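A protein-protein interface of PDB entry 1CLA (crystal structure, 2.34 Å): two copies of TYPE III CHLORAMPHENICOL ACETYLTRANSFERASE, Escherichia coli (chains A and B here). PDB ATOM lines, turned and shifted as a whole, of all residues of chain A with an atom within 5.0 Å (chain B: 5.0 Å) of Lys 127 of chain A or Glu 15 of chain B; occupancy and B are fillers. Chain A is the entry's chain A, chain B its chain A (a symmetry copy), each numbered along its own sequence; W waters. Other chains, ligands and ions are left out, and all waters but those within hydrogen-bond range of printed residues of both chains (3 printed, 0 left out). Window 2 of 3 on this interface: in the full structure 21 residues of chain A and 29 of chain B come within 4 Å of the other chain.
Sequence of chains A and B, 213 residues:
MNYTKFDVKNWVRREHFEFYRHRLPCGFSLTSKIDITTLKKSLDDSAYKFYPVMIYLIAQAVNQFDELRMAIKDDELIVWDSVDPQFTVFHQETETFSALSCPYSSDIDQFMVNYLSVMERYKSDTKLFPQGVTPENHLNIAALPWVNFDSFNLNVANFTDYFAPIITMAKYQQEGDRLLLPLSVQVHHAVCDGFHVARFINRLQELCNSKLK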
ATOM      1  N   PHE A  97     -29.132   4.894  20.212  1.00  0.00           N
ATOM      2  CA  PHE A  97     -30.226   4.118  20.800  1.00  0.00           C
ATOM      3  C   PHE A  97     -30.456   2.847  19.981  1.00  0.00           C
ATOM      4  O   PHE A  97     -30.071   2.756  18.808  1.00  0.00           O
ATOM      5  CB  PHE A  97     -31.511   4.958  20.899  1.00  0.00           C
ATOM      6  CG  PHE A  97     -32.260   5.239  19.638  1.00  0.00           C
ATOM      7  CD1 PHE A  97     -33.340   4.421  19.278  1.00  0.00           C
ATOM      8  CD2 PHE A  97     -31.869   6.277  18.800  1.00  0.00           C
ATOM      9  CE1 PHE A  97     -34.036   4.638  18.100  1.00  0.00           C
ATOM     10  CE2 PHE A  97     -32.565   6.498  17.610  1.00  0.00           C
ATOM     11  CZ  PHE A  97     -33.674   5.718  17.285  1.00  0.00           C
ATOM     12  N   SER A  98     -31.122   1.938  20.649  1.00  0.00           N
ATOM     13  CA  SER A  98     -31.568   0.636  20.056  1.00  0.00           C
ATOM     14  C   SER A  98     -33.052   0.625  20.463  1.00  0.00           C
ATOM     15  O   SER A  98     -33.430   1.379  21.396  1.00  0.00           O
ATOM     16  CB  SER A  98     -30.821  -0.546  20.598  1.00  0.00           C
ATOM     17  OG  SER A  98     -29.457  -0.587  20.250  1.00  0.00           O
ATOM     18  N   ASP A 125     -25.586  -4.185  22.867  1.00  0.00           N
ATOM     19  CA  ASP A 125     -25.846  -4.413  21.443  1.00  0.00           C
ATOM     20  C   ASP A 125     -26.308  -3.100  20.825  1.00  0.00           C
ATOM     21  O   ASP A 125     -27.497  -2.741  20.921  1.00  0.00           O
ATOM     22  CB  ASP A 125     -26.857  -5.554  21.222  1.00  0.00           C
ATOM     23  CG  ASP A 125     -26.824  -6.047  19.791  1.00  0.00           C
ATOM     24  OD1 ASP A 125     -26.690  -5.278  18.811  1.00  0.00           O
ATOM     25  OD2 ASP A 125     -26.946  -7.280  19.647  1.00  0.00           O
ATOM     26  N   THR A 126     -25.400  -2.511  20.037  1.00  0.00           N
ATOM     27  CA  THR A 126     -25.678  -1.258  19.366  1.00  0.00           C
ATOM     28  C   THR A 126     -26.417  -1.362  18.017  1.00  0.00           C
ATOM     29  O   THR A 126     -26.572  -0.346  17.314  1.00  0.00           O
ATOM     30  CB  THR A 126     -24.383  -0.466  19.178  1.00  0.00           C
ATOM     31  OG1 THR A 126     -23.533  -1.131  18.265  1.00  0.00           O
ATOM     32  CG2 THR A 126     -23.617  -0.281  20.498  1.00  0.00           C
ATOM     33  N   LYS A 127     -26.900  -2.549  17.592  1.00  0.00           N
ATOM     34  CA  LYS A 127     -27.726  -2.533  16.352  1.00  0.00           C
ATOM     35  C   LYS A 127     -28.987  -1.778  16.681  1.00  0.00           C
ATOM     36  O   LYS A 127     -29.386  -1.664  17.851  1.00  0.00           O
ATOM     37  CB  LYS A 127     -28.215  -3.898  15.720  1.00  0.00           C
ATOM     38  CG  LYS A 127     -26.948  -4.880  15.527  1.00  0.00           C
ATOM     39  CD  LYS A 127     -27.177  -6.419  15.155  1.00  0.00           C
ATOM     40  N   LEU A 128     -29.599  -1.261  15.653  1.00  0.00           N
ATOM     41  CA  LEU A 128     -30.830  -0.502  15.818  1.00  0.00           C
ATOM     42  C   LEU A 128     -31.925  -1.421  16.347  1.00  0.00           C
ATOM     43  O   LEU A 128     -32.722  -1.009  17.232  1.00  0.00           O
ATOM     44  CB  LEU A 128     -31.246   0.123  14.490  1.00  0.00           C
ATOM     45  CG  LEU A 128     -32.557   0.912  14.574  1.00  0.00           C
ATOM     46  CD1 LEU A 128     -32.605   1.897  15.747  1.00  0.00           C
ATOM     47  CD2 LEU A 128     -32.820   1.741  13.317  1.00  0.00           C
ATOM     48  N   PHE A 129     -32.069  -2.624  15.897  1.00  0.00           N
ATOM     49  CA  PHE A 129     -32.983  -3.705  16.235  1.00  0.00           C
ATOM     50  C   PHE A 129     -32.155  -4.999  16.501  1.00  0.00           C
ATOM     51  O   PHE A 129     -32.121  -5.864  15.600  1.00  0.00           O
ATOM     52  CB  PHE A 129     -34.052  -4.022  15.175  1.00  0.00           C
ATOM     53  CG  PHE A 129     -34.828  -2.832  14.681  1.00  0.00           C
ATOM     54  CD1 PHE A 129     -34.529  -2.261  13.435  1.00  0.00           C
ATOM     55  CD2 PHE A 129     -35.835  -2.253  15.441  1.00  0.00           C
ATOM     56  CE1 PHE A 129     -35.188  -1.165  12.979  1.00  0.00           C
ATOM     57  CE2 PHE A 129     -36.523  -1.163  14.973  1.00  0.00           C
ATOM     58  CZ  PHE A 129     -36.197  -0.562  13.749  1.00  0.00           C
ATOM     59  N   PRO A 130     -31.603  -5.055  17.733  1.00  0.00           N
ATOM     60  CA  PRO A 130     -30.775  -6.181  18.204  1.00  0.00           C
ATOM     61  C   PRO A 130     -31.397  -7.555  18.052  1.00  0.00           C
ATOM     62  O   PRO A 130     -30.788  -8.536  17.573  1.00  0.00           O
ATOM     63  CB  PRO A 130     -30.378  -5.872  19.664  1.00  0.00           C
ATOM     64  CG  PRO A 130     -30.544  -4.371  19.735  1.00  0.00           C
ATOM     65  CD  PRO A 130     -31.666  -4.021  18.794  1.00  0.00           C
ATOM     66  N   ARG B  13     -23.968   5.746  14.247  1.00  0.00           N
ATOM     67  CA  ARG B  13     -25.342   6.047  13.807  1.00  0.00           C
ATOM     68  C   ARG B  13     -25.508   5.811  12.305  1.00  0.00           C
ATOM     69  O   ARG B  13     -26.471   6.239  11.650  1.00  0.00           O
ATOM     70  CB  ARG B  13     -25.638   7.533  14.046  1.00  0.00           C
ATOM     71  CG  ARG B  13     -25.874   7.953  15.450  1.00  0.00           C
ATOM     72  CD  ARG B  13     -26.531   9.266  15.582  1.00  0.00           C
ATOM     73  NE  ARG B  13     -27.938   9.305  15.310  1.00  0.00           N
ATOM     74  CZ  ARG B  13     -28.496   9.572  14.143  1.00  0.00           C
ATOM     75  NH1 ARG B  13     -27.727   9.813  13.061  1.00  0.00           N
ATOM     76  NH2 ARG B  13     -29.851   9.596  14.043  1.00  0.00           N
ATOM     77  N   ARG B  14     -24.625   4.996  11.678  1.00  0.00           N
ATOM     78  CA  ARG B  14     -24.736   4.775  10.255  1.00  0.00           C
ATOM     79  C   ARG B  14     -25.959   3.990   9.902  1.00  0.00           C
ATOM     80  O   ARG B  14     -26.518   4.128   8.801  1.00  0.00           O
ATOM     81  CB  ARG B  14     -23.475   4.208   9.637  1.00  0.00           C
ATOM     82  CG  ARG B  14     -23.130   2.800   9.966  1.00  0.00           C
ATOM     83  CD  ARG B  14     -21.954   2.366   9.122  1.00  0.00           C
ATOM     84  NE  ARG B  14     -21.418   1.031   9.420  1.00  0.00           N
ATOM     85  CZ  ARG B  14     -20.924   0.680  10.608  1.00  0.00           C
ATOM     86  NH1 ARG B  14     -20.904   1.544  11.631  1.00  0.00           N
ATOM     87  NH2 ARG B  14     -20.407  -0.542  10.862  1.00  0.00           N
ATOM     88  N   GLU B  15     -26.372   3.074  10.752  1.00  0.00           N
ATOM     89  CA  GLU B  15     -27.584   2.275  10.456  1.00  0.00           C
ATOM     90  C   GLU B  15     -28.779   3.179  10.616  1.00  0.00           C
ATOM     91  O   GLU B  15     -29.695   3.216   9.773  1.00  0.00           O
ATOM     92  CB  GLU B  15     -27.662   1.006  11.338  1.00  0.00           C
ATOM     93  CG  GLU B  15     -28.727   0.013  10.981  1.00  0.00           C
ATOM     94  CD  GLU B  15     -29.103  -0.955  12.066  1.00  0.00           C
ATOM     95  OE1 GLU B  15     -28.515  -1.030  13.096  1.00  0.00           O
ATOM     96  OE2 GLU B  15     -30.081  -1.700  11.734  1.00  0.00           O
ATOM     97  N   HIS B  16     -28.812   4.021  11.640  1.00  0.00           N
ATOM     98  CA  HIS B  16     -29.825   5.016  11.929  1.00  0.00           C
ATOM     99  C   HIS B  16     -30.069   6.008  10.797  1.00  0.00           C
ATOM    100  O   HIS B  16     -31.167   6.441  10.391  1.00  0.00           O
ATOM    101  CB  HIS B  16     -29.318   5.875  13.159  1.00  0.00           C
ATOM    102  CG  HIS B  16     -29.122   4.970  14.345  1.00  0.00           C
ATOM    103  ND1 HIS B  16     -28.083   4.143  14.517  1.00  0.00           N
ATOM    104  CD2 HIS B  16     -29.945   4.728  15.394  1.00  0.00           C
ATOM    105  CE1 HIS B  16     -28.235   3.442  15.651  1.00  0.00           C
ATOM    106  NE2 HIS B  16     -29.363   3.814  16.213  1.00  0.00           N
ATOM    107  N   PHE B  17     -28.953   6.502  10.277  1.00  0.00           N
ATOM    108  CA  PHE B  17     -28.850   7.482   9.193  1.00  0.00           C
ATOM    109  C   PHE B  17     -29.606   6.975   7.980  1.00  0.00           C
ATOM    110  O   PHE B  17     -30.551   7.635   7.546  1.00  0.00           O
ATOM    111  CB  PHE B  17     -27.383   7.853   8.942  1.00  0.00           C
ATOM    112  CG  PHE B  17     -27.256   8.757   7.773  1.00  0.00           C
ATOM    113  CD1 PHE B  17     -26.698   8.265   6.606  1.00  0.00           C
ATOM    114  CD2 PHE B  17     -27.685  10.080   7.924  1.00  0.00           C
ATOM    115  CE1 PHE B  17     -26.600   9.114   5.505  1.00  0.00           C
ATOM    116  CE2 PHE B  17     -27.526  10.945   6.820  1.00  0.00           C
ATOM    117  CZ  PHE B  17     -26.980  10.464   5.613  1.00  0.00           C
ATOM    118  N   GLU B  18     -29.267   5.777   7.496  1.00  0.00           N
ATOM    119  CA  GLU B  18     -29.984   5.175   6.344  1.00  0.00           C
ATOM    120  C   GLU B  18     -31.393   4.853   6.743  1.00  0.00           C
ATOM    121  O   GLU B  18     -32.341   5.032   5.947  1.00  0.00           O
ATOM    122  CB  GLU B  18     -29.295   3.885   5.897  1.00  0.00           C
ATOM    123  CG  GLU B  18     -29.773   3.137   4.677  1.00  0.00           C
ATOM    124  CD  GLU B  18     -29.828   3.750   3.315  1.00  0.00           C
ATOM    125  OE1 GLU B  18     -30.558   3.392   2.377  1.00  0.00           O
ATOM    126  OE2 GLU B  18     -29.118   4.774   3.195  1.00  0.00           O
ATOM    127  N   PHE B  19     -31.642   4.360   7.968  1.00  0.00           N
ATOM    128  CA  PHE B  19     -33.024   4.014   8.364  1.00  0.00           C
ATOM    129  C   PHE B  19     -33.986   5.181   8.206  1.00  0.00           C
ATOM    130  O   PHE B  19     -35.000   5.140   7.481  1.00  0.00           O
ATOM    131  CB  PHE B  19     -33.101   3.509   9.822  1.00  0.00           C
ATOM    132  CG  PHE B  19     -34.454   2.958  10.159  1.00  0.00           C
ATOM    133  CD1 PHE B  19     -35.299   3.730  10.946  1.00  0.00           C
ATOM    134  CD2 PHE B  19     -34.874   1.709   9.731  1.00  0.00           C
ATOM    135  CE1 PHE B  19     -36.559   3.260  11.314  1.00  0.00           C
ATOM    136  CE2 PHE B  19     -36.149   1.220  10.083  1.00  0.00           C
ATOM    137  CZ  PHE B  19     -36.989   1.988  10.854  1.00  0.00           C
HETATM  138  O   HOH W   1     -26.354   0.315  14.681  1.00  0.00           O
HETATM  139  O   HOH W   2     -28.430   6.273  17.377  1.00  0.00           O
HETATM  140  O   HOH W   3     -30.642  -3.504  13.373  1.00  0.00           O
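NE2 of His 16 of chain B is in hydrogen-bond range of O of Phe 97 of chain A (2.9 Å). The side-chain carboxylate (OE1) of Glu 15 of chain B lies within hydrogen-bond range of the backbone NH (N) of Leu 128 of chain A, 2.8 Å away.
The side-chain hydroxyl (OG) of Ser 98 of chain A is in hydrogen-bond range of the backbone carbonyl oxygen (O) of Lys 127 of chain A (2.6 Å). The side-chain carboxylate (OD1) of Asp 125 of chain A sits at hydrogen-bond distance from the backbone NH (N) of Lys 127 of chain A, 3.0 Å away.
Glu 15 of chain B touches Lys 127 of chain A (OE1 to CA, 3.7 Å). His 16 of chain B touches Leu 128 of chain A (NE2 to CD1, 3.8 Å). CD2 of Leu 128 of chain A touches CG of Phe 19 of chain B (3.8 Å). CE1 of Phe 129 of chain A touches CE2 of Phe 19 of chain B (3.9 Å).
Of chain B, only Glu 15 comes within 4 Å of Lys 127 of chain A. Of the printed residues of chain B, Leu 128 of chain A touches Glu 15 (2.8 Å), His 16 (3.8 Å) and Phe 19 (3.8 Å). Printed residues of chain B within 4 Å of Phe 129 of chain A: Phe 19 (3.9 Å). Pro 130 of chain A touches none of the printed residues of chain B. Of the printed residues of chain A, His 16 of chain B touches Phe 97 (2.9 Å) and Leu 128 (3.8 Å). Phe 17 of chain B touches none of the printed residues of chain A. Of the printed residues of chain A, Phe 19 of chain B touches Leu 128 (3.8 Å) and Phe 129 (3.9 Å).
Hydrophobic or aromatic side chains of chain A within 4 Å of the printed part of chain B: Phe 97, Leu 128 and Phe 129. Of the 7 printed residues of chain B, 3 touch a printed residue of chain A. Hydrophobic or aromatic side chains of chain B within 4 Å of the printed part of chain A: His 16 and Phe 19.
No position is printed for both chains.
Water W3 lies within hydrogen-bond range of OE2 of Glu 15 of chain B, N of Phe 129 of chain A and N of Leu 128 of chain A. Water W1 bridges the backbone carbonyl oxygen (O) of Thr 126 of chain A (2.7 Å) and the side-chain carboxylate (OE1) of Glu 15 of chain B (3.0 Å). Water W2 lies within hydrogen-bond range of NE2 of His 16 of chain B and N of Phe 97 of chain A.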
